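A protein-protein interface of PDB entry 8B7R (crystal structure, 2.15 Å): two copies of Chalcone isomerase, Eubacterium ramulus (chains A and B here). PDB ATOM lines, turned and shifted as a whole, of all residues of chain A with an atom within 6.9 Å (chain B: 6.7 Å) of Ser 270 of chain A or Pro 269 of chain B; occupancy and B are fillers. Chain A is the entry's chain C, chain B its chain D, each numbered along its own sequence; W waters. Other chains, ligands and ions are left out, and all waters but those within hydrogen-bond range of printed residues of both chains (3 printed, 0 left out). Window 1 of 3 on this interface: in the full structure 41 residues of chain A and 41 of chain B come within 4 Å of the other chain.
Printed residues of chain B within 4 Å of Tyr 31 of chain A: Tyr 267.
Printed residues of chain B within 4 Å of Pro 269 of chain A: Ser 270.
Ser 270 of chain A touches one residue of chain B.
Phe 51 of chain B touches none of the printed residues of chain A.
Of the printed residues of chain A, Tyr 267 of chain B touches Tyr 31 (3.5 Å).
Of the printed residues of chain A, Asn 275 of chain B touches Asn 275 (3.5 Å).
Printed residues of chain A within 4 Å of Tyr 276 of chain B: Tyr 267.
The nearest residue of chain A that does not touch Pro 269 of chain B is Pro 269 of chain A (4.1 Å).
The side-chain hydroxyl (OH) of Tyr 31 of chain A lies within hydrogen-bond range of the side-chain hydroxyl (OG) of Ser 270 of chain A, 3.2 Å away.
The side-chain hydroxyl (OG1) of Thr 268 of chain B is in hydrogen-bond range of the backbone NH (N) of Ser 270 of chain B (3.0 Å).
OG1 of Thr 268 of chain A sits at hydrogen-bond distance from N of Ser 270 of chain A (3.0 Å).
The side-chain amide nitrogen (ND2) of Asn 275 of chain B is in hydrogen-bond range of the backbone carbonyl oxygen (O) of Pro 269 of chain B (2.9 Å).
The backbone carbonyl oxygen (O) of Ser 270 of chain B is in hydrogen-bond range of the backbone NH (N) of Phe 51 of chain B (3.0 Å).
The backbone NH (N) of Phe 51 of chain A lies within hydrogen-bond range of the backbone carbonyl oxygen (O) of Ser 270 of chain A (3.0 Å).
Water W1 lies within hydrogen-bond range of the backbone carbonyl oxygen (O) of Tyr 267 of chain B (2.8 Å) and the side-chain amide nitrogen (NE2) of Gln 27 of chain A (3.1 Å).
Water W2 bridges O of Asn 275 of chain B (3.0 Å) and OD1 of Asn 275 of chain A (3.5 Å).
Water W3 bridges OH of Tyr 267 of chain B (3.2 Å) and OD1 of Asn 272 of chain A (3.4 Å).
CD1 of Tyr 31 of chain A touches CE2 of Tyr 267 of chain B (3.5 Å).
Tyr 267 of chain A touches Tyr 276 of chain B.
CB of Pro 269 of chain A touches OG of Ser 270 of chain B, 3.5 Å away.
Pro 269 of chain B touches Ser 270 of chain A.
Asn 275 of chain A touches Asn 275 of chain B (O to CG, 3.5 Å).
Pro 269 of chain A touches Ser 270 of chain B, and with the chains exchanged Ser 270 of chain A touches Pro 269 of chain B.
Asn 275 of chain B touches its own counterpart, Asn 275 of chain A.
Hydrophobic or aromatic side chains of chain B that line the printed part of chain A: Tyr 267, Pro 269 and Tyr 276.
Of the 17 printed residues of chain A, 5 touch a printed residue of chain B.
Printed residues of chain A that touch a printed residue of chain B: Tyr 31, Tyr 267, Pro 269, Ser 270 and Asn 275.
Hydrophobic or aromatic side chains of chain A within 4 Å of the printed part of chain B: Tyr 31, Tyr 267 and Pro 269.
Among the printed residues, no Asp or Glu carboxylate lies within 4 Å of a Lys or Arg side-chain nitrogen of the other chain.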
ATOM      1  N   GLN A  27      12.397  22.303  16.739  1.00  0.00           N
ATOM      2  CA  GLN A  27      11.806  21.226  17.523  1.00  0.00           C
ATOM      3  C   GLN A  27      11.979  19.881  16.811  1.00  0.00           C
ATOM      4  O   GLN A  27      12.305  18.870  17.432  1.00  0.00           O
ATOM      5  CB  GLN A  27      10.341  21.561  17.784  1.00  0.00           C
ATOM      6  CG  GLN A  27       9.700  20.708  18.882  1.00  0.00           C
ATOM      7  CD  GLN A  27       8.448  21.339  19.444  1.00  0.00           C
ATOM      8  OE1 GLN A  27       8.481  22.480  19.897  1.00  0.00           O
ATOM      9  NE2 GLN A  27       7.330  20.636  19.384  1.00  0.00           N
ATOM     10  N   TYR A  31      14.158  16.637  18.354  1.00  0.00           N
ATOM     11  CA  TYR A  31      13.513  15.375  18.710  1.00  0.00           C
ATOM     12  C   TYR A  31      13.776  14.283  17.680  1.00  0.00           C
ATOM     13  O   TYR A  31      13.741  13.085  18.010  1.00  0.00           O
ATOM     14  CB  TYR A  31      12.018  15.593  18.945  1.00  0.00           C
ATOM     15  CG  TYR A  31      11.731  16.224  20.287  1.00  0.00           C
ATOM     16  CD1 TYR A  31      11.618  15.447  21.429  1.00  0.00           C
ATOM     17  CD2 TYR A  31      11.647  17.595  20.435  1.00  0.00           C
ATOM     18  CE1 TYR A  31      11.401  16.016  22.679  1.00  0.00           C
ATOM     19  CE2 TYR A  31      11.417  18.180  21.681  1.00  0.00           C
ATOM     20  CZ  TYR A  31      11.293  17.386  22.811  1.00  0.00           C
ATOM     21  OH  TYR A  31      11.109  17.933  24.058  1.00  0.00           O
ATOM     22  N   ILE A  35      18.320  13.799  19.434  1.00  0.00           N
ATOM     23  CA  ILE A  35      18.202  12.795  20.490  1.00  0.00           C
ATOM     24  C   ILE A  35      19.017  11.544  20.145  1.00  0.00           C
ATOM     25  O   ILE A  35      19.862  11.101  20.922  1.00  0.00           O
ATOM     26  CB  ILE A  35      16.740  12.453  20.823  1.00  0.00           C
ATOM     27  CG1 ILE A  35      16.075  13.589  21.611  1.00  0.00           C
ATOM     28  CG2 ILE A  35      16.661  11.167  21.618  1.00  0.00           C
ATOM     29  CD1 ILE A  35      14.597  13.328  21.924  1.00  0.00           C
ATOM     30  N   LYS A  48      21.360  10.204  32.770  1.00  0.00           N
ATOM     31  CA  LYS A  48      20.081  10.846  32.525  1.00  0.00           C
ATOM     32  C   LYS A  48      20.273  11.974  31.510  1.00  0.00           C
ATOM     33  O   LYS A  48      21.252  12.715  31.567  1.00  0.00           O
ATOM     34  CB  LYS A  48      19.483  11.365  33.837  1.00  0.00           C
ATOM     35  CG  LYS A  48      18.054  11.866  33.748  1.00  0.00           C
ATOM     36  CD  LYS A  48      17.581  12.451  35.065  1.00  0.00           C
ATOM     37  CE  LYS A  48      16.231  13.141  34.953  1.00  0.00           C
ATOM     38  NZ  LYS A  48      15.147  12.151  34.704  1.00  0.00           N
ATOM     39  N   TYR A  49      19.304  12.068  30.584  1.00  0.00           N
ATOM     40  CA  TYR A  49      19.302  13.014  29.480  1.00  0.00           C
ATOM     41  C   TYR A  49      17.854  13.430  29.256  1.00  0.00           C
ATOM     42  O   TYR A  49      17.045  12.596  28.872  1.00  0.00           O
ATOM     43  CB  TYR A  49      19.885  12.328  28.245  1.00  0.00           C
ATOM     44  CG  TYR A  49      19.836  13.091  26.945  1.00  0.00           C
ATOM     45  CD1 TYR A  49      20.115  14.450  26.862  1.00  0.00           C
ATOM     46  CD2 TYR A  49      19.575  12.430  25.759  1.00  0.00           C
ATOM     47  CE1 TYR A  49      20.127  15.117  25.646  1.00  0.00           C
ATOM     48  CE2 TYR A  49      19.589  13.086  24.527  1.00  0.00           C
ATOM     49  CZ  TYR A  49      19.858  14.427  24.469  1.00  0.00           C
ATOM     50  OH  TYR A  49      19.799  15.026  23.245  1.00  0.00           O
ATOM     51  N   ALA A  50      17.531  14.695  29.524  1.00  0.00           N
ATOM     52  CA  ALA A  50      16.143  15.140  29.595  1.00  0.00           C
ATOM     53  C   ALA A  50      16.003  16.555  29.053  1.00  0.00           C
ATOM     54  O   ALA A  50      16.928  17.340  29.119  1.00  0.00           O
ATOM     55  CB  ALA A  50      15.646  15.062  31.028  1.00  0.00           C
ATOM     56  N   PHE A  51      14.847  16.821  28.454  1.00  0.00           N
ATOM     57  CA  PHE A  51      14.489  18.149  27.993  1.00  0.00           C
ATOM     58  C   PHE A  51      13.308  18.647  28.794  1.00  0.00           C
ATOM     59  O   PHE A  51      12.366  17.905  28.993  1.00  0.00           O
ATOM     60  CB  PHE A  51      14.040  18.139  26.528  1.00  0.00           C
ATOM     61  CG  PHE A  51      15.015  17.568  25.540  1.00  0.00           C
ATOM     62  CD1 PHE A  51      16.389  17.648  25.740  1.00  0.00           C
ATOM     63  CD2 PHE A  51      14.554  16.991  24.372  1.00  0.00           C
ATOM     64  CE1 PHE A  51      17.279  17.155  24.792  1.00  0.00           C
ATOM     65  CE2 PHE A  51      15.451  16.496  23.426  1.00  0.00           C
ATOM     66  CZ  PHE A  51      16.805  16.577  23.639  1.00  0.00           C
ATOM     67  N   TYR A  52      13.393  19.894  29.252  1.00  0.00           N
ATOM     68  CA  TYR A  52      12.331  20.554  29.996  1.00  0.00           C
ATOM     69  C   TYR A  52      11.866  21.743  29.167  1.00  0.00           C
ATOM     70  O   TYR A  52      12.493  22.802  29.150  1.00  0.00           O
ATOM     71  CB  TYR A  52      12.783  20.948  31.410  1.00  0.00           C
ATOM     72  CG  TYR A  52      13.281  19.797  32.249  1.00  0.00           C
ATOM     73  CD1 TYR A  52      14.587  19.354  32.111  1.00  0.00           C
ATOM     74  CD2 TYR A  52      12.447  19.113  33.128  1.00  0.00           C
ATOM     75  CE1 TYR A  52      15.071  18.297  32.868  1.00  0.00           C
ATOM     76  CE2 TYR A  52      12.910  18.016  33.861  1.00  0.00           C
ATOM     77  CZ  TYR A  52      14.240  17.614  33.746  1.00  0.00           C
ATOM     78  OH  TYR A  52      14.780  16.535  34.443  1.00  0.00           O
ATOM     79  N   PRO A  53      10.738  21.584  28.436  1.00  0.00           N
ATOM     80  CA  PRO A  53      10.181  22.639  27.585  1.00  0.00           C
ATOM     81  C   PRO A  53       9.843  23.850  28.442  1.00  0.00           C
ATOM     82  O   PRO A  53       9.303  23.699  29.551  1.00  0.00           O
ATOM     83  CB  PRO A  53       8.859  22.065  27.038  1.00  0.00           C
ATOM     84  CG  PRO A  53       8.997  20.617  27.226  1.00  0.00           C
ATOM     85  CD  PRO A  53       9.901  20.370  28.418  1.00  0.00           C
ATOM     86  N   TYR A 267       7.643  18.122  35.982  1.00  0.00           N
ATOM     87  CA  TYR A 267       7.724  16.885  35.227  1.00  0.00           C
ATOM     88  C   TYR A 267       7.946  17.206  33.745  1.00  0.00           C
ATOM     89  O   TYR A 267       7.362  18.171  33.219  1.00  0.00           O
ATOM     90  CB  TYR A 267       6.395  16.131  35.369  1.00  0.00           C
ATOM     91  CG  TYR A 267       6.212  14.955  34.444  1.00  0.00           C
ATOM     92  CD1 TYR A 267       6.800  13.724  34.720  1.00  0.00           C
ATOM     93  CD2 TYR A 267       5.487  15.074  33.255  1.00  0.00           C
ATOM     94  CE1 TYR A 267       6.652  12.634  33.864  1.00  0.00           C
ATOM     95  CE2 TYR A 267       5.332  13.992  32.403  1.00  0.00           C
ATOM     96  CZ  TYR A 267       5.916  12.771  32.705  1.00  0.00           C
ATOM     97  OH  TYR A 267       5.780  11.702  31.872  1.00  0.00           O
ATOM     98  N   THR A 268       8.745  16.354  33.072  1.00  0.00           N
ATOM     99  CA  THR A 268       8.819  16.344  31.618  1.00  0.00           C
ATOM    100  C   THR A 268       8.607  14.927  31.101  1.00  0.00           C
ATOM    101  O   THR A 268       9.140  13.954  31.634  1.00  0.00           O
ATOM    102  CB  THR A 268      10.163  16.827  31.032  1.00  0.00           C
ATOM    103  OG1 THR A 268      10.076  16.814  29.602  1.00  0.00           O
ATOM    104  CG2 THR A 268      11.326  15.951  31.460  1.00  0.00           C
ATOM    105  N   PRO A 269       7.830  14.780  30.021  1.00  0.00           N
ATOM    106  CA  PRO A 269       7.739  13.504  29.309  1.00  0.00           C
ATOM    107  C   PRO A 269       9.012  13.165  28.533  1.00  0.00           C
ATOM    108  O   PRO A 269       9.243  12.014  28.203  1.00  0.00           O
ATOM    109  CB  PRO A 269       6.545  13.700  28.378  1.00  0.00           C
ATOM    110  CG  PRO A 269       6.419  15.176  28.191  1.00  0.00           C
ATOM    111  CD  PRO A 269       6.963  15.819  29.453  1.00  0.00           C
ATOM    112  N   SER A 270       9.891  14.151  28.337  1.00  0.00           N
ATOM    113  CA  SER A 270      11.113  13.957  27.579  1.00  0.00           C
ATOM    114  C   SER A 270      12.280  13.580  28.489  1.00  0.00           C
ATOM    115  O   SER A 270      13.271  14.294  28.586  1.00  0.00           O
ATOM    116  CB  SER A 270      11.399  15.171  26.739  1.00  0.00           C
ATOM    117  OG  SER A 270      10.370  15.336  25.765  1.00  0.00           O
ATOM    118  N   ASN A 271      12.150  12.421  29.132  1.00  0.00           N
ATOM    119  CA  ASN A 271      13.238  11.738  29.808  1.00  0.00           C
ATOM    120  C   ASN A 271      13.826  10.725  28.827  1.00  0.00           C
ATOM    121  O   ASN A 271      13.407   9.577  28.767  1.00  0.00           O
ATOM    122  CB  ASN A 271      12.766  11.071  31.106  1.00  0.00           C
ATOM    123  CG  ASN A 271      13.916  10.590  31.962  1.00  0.00           C
ATOM    124  OD1 ASN A 271      14.992  11.177  31.919  1.00  0.00           O
ATOM    125  ND2 ASN A 271      13.703   9.549  32.755  1.00  0.00           N
ATOM    126  N   ASN A 272      14.824  11.170  28.073  1.00  0.00           N
ATOM    127  CA  ASN A 272      15.112  10.613  26.761  1.00  0.00           C
ATOM    128  C   ASN A 272      15.765   9.236  26.841  1.00  0.00           C
ATOM    129  O   ASN A 272      15.523   8.402  25.965  1.00  0.00           O
ATOM    130  CB  ASN A 272      15.986  11.557  25.940  1.00  0.00           C
ATOM    131  CG  ASN A 272      15.309  12.894  25.694  1.00  0.00           C
ATOM    132  OD1 ASN A 272      14.100  12.919  25.448  1.00  0.00           O
ATOM    133  ND2 ASN A 272      16.077  13.978  25.722  1.00  0.00           N
ATOM    134  N   LEU A 273      16.570   8.966  27.867  1.00  0.00           N
ATOM    135  CA  LEU A 273      17.186   7.652  27.948  1.00  0.00           C
ATOM    136  C   LEU A 273      16.158   6.601  28.319  1.00  0.00           C
ATOM    137  O   LEU A 273      16.372   5.444  27.992  1.00  0.00           O
ATOM    138  CB  LEU A 273      18.337   7.603  28.948  1.00  0.00           C
ATOM    139  CG  LEU A 273      19.570   8.373  28.518  1.00  0.00           C
ATOM    140  CD1 LEU A 273      20.617   8.323  29.610  1.00  0.00           C
ATOM    141  CD2 LEU A 273      20.136   7.827  27.241  1.00  0.00           C
ATOM    142  N   ASN A 275      12.514   7.024  27.672  1.00  0.00           N
ATOM    143  CA  ASN A 275      11.163   7.232  27.163  1.00  0.00           C
ATOM    144  C   ASN A 275      11.152   7.311  25.629  1.00  0.00           C
ATOM    145  O   ASN A 275      10.070   7.260  25.041  1.00  0.00           O
ATOM    146  CB  ASN A 275      10.475   8.507  27.743  1.00  0.00           C
ATOM    147  CG  ASN A 275      10.179   8.509  29.247  1.00  0.00           C
ATOM    148  OD1 ASN A 275      10.412   7.522  29.955  1.00  0.00           O
ATOM    149  ND2 ASN A 275       9.656   9.615  29.766  1.00  0.00           N
ATOM    150  N   PHE B  51      -1.107  12.916  24.022  1.00  0.00           N
ATOM    151  CA  PHE B  51      -1.341  14.343  24.162  1.00  0.00           C
ATOM    152  C   PHE B  51      -0.427  15.078  23.198  1.00  0.00           C
ATOM    153  O   PHE B  51       0.738  14.742  23.105  1.00  0.00           O
ATOM    154  CB  PHE B  51      -0.996  14.840  25.563  1.00  0.00           C
ATOM    155  CG  PHE B  51      -1.701  14.156  26.698  1.00  0.00           C
ATOM    156  CD1 PHE B  51      -2.981  13.641  26.552  1.00  0.00           C
ATOM    157  CD2 PHE B  51      -1.094  14.073  27.944  1.00  0.00           C
ATOM    158  CE1 PHE B  51      -3.633  13.048  27.634  1.00  0.00           C
ATOM    159  CE2 PHE B  51      -1.756  13.472  29.020  1.00  0.00           C
ATOM    160  CZ  PHE B  51      -3.038  12.983  28.874  1.00  0.00           C
ATOM    161  N   PRO B  53       0.759  18.804  22.835  1.00  0.00           N
ATOM    162  CA  PRO B  53       0.817  20.159  23.384  1.00  0.00           C
ATOM    163  C   PRO B  53       0.675  21.179  22.263  1.00  0.00           C
ATOM    164  O   PRO B  53       1.250  21.018  21.188  1.00  0.00           O
ATOM    165  CB  PRO B  53       2.222  20.317  23.989  1.00  0.00           C
ATOM    166  CG  PRO B  53       2.842  18.924  23.983  1.00  0.00           C
ATOM    167  CD  PRO B  53       1.998  18.040  23.086  1.00  0.00           C
ATOM    168  N   TYR B 267       5.301  15.402  16.062  1.00  0.00           N
ATOM    169  CA  TYR B 267       5.700  14.424  17.064  1.00  0.00           C
ATOM    170  C   TYR B 267       5.289  14.903  18.445  1.00  0.00           C
ATOM    171  O   TYR B 267       5.363  16.100  18.725  1.00  0.00           O
ATOM    172  CB  TYR B 267       7.221  14.217  17.007  1.00  0.00           C
ATOM    173  CG  TYR B 267       7.839  13.490  18.177  1.00  0.00           C
ATOM    174  CD1 TYR B 267       7.842  12.108  18.214  1.00  0.00           C
ATOM    175  CD2 TYR B 267       8.377  14.162  19.273  1.00  0.00           C
ATOM    176  CE1 TYR B 267       8.383  11.401  19.277  1.00  0.00           C
ATOM    177  CE2 TYR B 267       8.924  13.467  20.341  1.00  0.00           C
ATOM    178  CZ  TYR B 267       8.935  12.082  20.338  1.00  0.00           C
ATOM    179  OH  TYR B 267       9.495  11.366  21.368  1.00  0.00           O
ATOM    180  N   THR B 268       4.904  13.966  19.321  1.00  0.00           N
ATOM    181  CA  THR B 268       4.743  14.226  20.745  1.00  0.00           C
ATOM    182  C   THR B 268       5.492  13.174  21.547  1.00  0.00           C
ATOM    183  O   THR B 268       5.436  11.991  21.258  1.00  0.00           O
ATOM    184  CB  THR B 268       3.290  14.224  21.251  1.00  0.00           C
ATOM    185  OG1 THR B 268       3.311  14.565  22.641  1.00  0.00           O
ATOM    186  CG2 THR B 268       2.606  12.894  21.079  1.00  0.00           C
ATOM    187  N   PRO B 269       6.209  13.598  22.602  1.00  0.00           N
ATOM    188  CA  PRO B 269       6.780  12.670  23.562  1.00  0.00           C
ATOM    189  C   PRO B 269       5.721  12.017  24.459  1.00  0.00           C
ATOM    190  O   PRO B 269       5.985  10.959  25.038  1.00  0.00           O
ATOM    191  CB  PRO B 269       7.771  13.512  24.361  1.00  0.00           C
ATOM    192  CG  PRO B 269       7.264  14.909  24.222  1.00  0.00           C
ATOM    193  CD  PRO B 269       6.542  14.994  22.900  1.00  0.00           C
ATOM    194  N   SER B 270       4.496  12.571  24.466  1.00  0.00           N
ATOM    195  CA  SER B 270       3.431  12.055  25.308  1.00  0.00           C
ATOM    196  C   SER B 270       2.563  11.050  24.564  1.00  0.00           C
ATOM    197  O   SER B 270       1.351  11.257  24.354  1.00  0.00           O
ATOM    198  CB  SER B 270       2.636  13.177  25.881  1.00  0.00           C
ATOM    199  OG  SER B 270       3.440  13.889  26.804  1.00  0.00           O
ATOM    200  N   ASN B 271       3.201   9.929  24.203  1.00  0.00           N
ATOM    201  CA  ASN B 271       2.496   8.738  23.735  1.00  0.00           C
ATOM    202  C   ASN B 271       2.293   7.809  24.933  1.00  0.00           C
ATOM    203  O   ASN B 271       3.134   6.975  25.232  1.00  0.00           O
ATOM    204  CB  ASN B 271       3.263   8.027  22.615  1.00  0.00           C
ATOM    205  CG  ASN B 271       2.411   7.007  21.910  1.00  0.00           C
ATOM    206  OD1 ASN B 271       1.187   7.136  21.860  1.00  0.00           O
ATOM    207  ND2 ASN B 271       3.058   6.014  21.331  1.00  0.00           N
ATOM    208  N   ASN B 272       1.162   7.978  25.615  1.00  0.00           N
ATOM    209  CA  ASN B 272       1.064   7.659  27.028  1.00  0.00           C
ATOM    210  C   ASN B 272       1.028   6.149  27.284  1.00  0.00           C
ATOM    211  O   ASN B 272       1.536   5.697  28.312  1.00  0.00           O
ATOM    212  CB  ASN B 272      -0.157   8.334  27.636  1.00  0.00           C
ATOM    213  CG  ASN B 272      -0.086   9.843  27.568  1.00  0.00           C
ATOM    214  OD1 ASN B 272       0.997  10.385  27.764  1.00  0.00           O
ATOM    215  ND2 ASN B 272      -1.218  10.502  27.328  1.00  0.00           N
ATOM    216  N   ASN B 275       4.923   5.315  26.825  1.00  0.00           N
ATOM    217  CA  ASN B 275       6.038   6.168  27.231  1.00  0.00           C
ATOM    218  C   ASN B 275       5.930   6.576  28.705  1.00  0.00           C
ATOM    219  O   ASN B 275       6.906   7.097  29.245  1.00  0.00           O
ATOM    220  CB  ASN B 275       6.167   7.455  26.361  1.00  0.00           C
ATOM    221  CG  ASN B 275       6.554   7.240  24.888  1.00  0.00           C
ATOM    222  OD1 ASN B 275       6.773   6.110  24.431  1.00  0.00           O
ATOM    223  ND2 ASN B 275       6.637   8.312  24.104  1.00  0.00           N
ATOM    224  N   TYR B 276       4.811   6.320  29.389  1.00  0.00           N
ATOM    225  CA  TYR B 276       4.619   6.870  30.729  1.00  0.00           C
ATOM    226  C   TYR B 276       5.271   5.994  31.798  1.00  0.00           C
ATOM    227  O   TYR B 276       5.025   4.792  31.802  1.00  0.00           O
ATOM    228  CB  TYR B 276       3.131   7.015  31.081  1.00  0.00           C
ATOM    229  CG  TYR B 276       2.822   7.778  32.352  1.00  0.00           C
ATOM    230  CD1 TYR B 276       3.066   9.146  32.459  1.00  0.00           C
ATOM    231  CD2 TYR B 276       2.254   7.134  33.446  1.00  0.00           C
ATOM    232  CE1 TYR B 276       2.755   9.844  33.611  1.00  0.00           C
ATOM    233  CE2 TYR B 276       1.953   7.821  34.619  1.00  0.00           C
ATOM    234  CZ  TYR B 276       2.186   9.182  34.692  1.00  0.00           C
ATOM    235  OH  TYR B 276       1.856   9.890  35.836  1.00  0.00           O
HETATM  236  O   HOH W   1       7.681  17.672  18.621  1.00  0.00           O
HETATM  237  O   HOH W   2       8.620   4.670  29.021  1.00  0.00           O
HETATM  238  O   HOH W   3      11.163  12.085  24.058  1.00  0.00           O
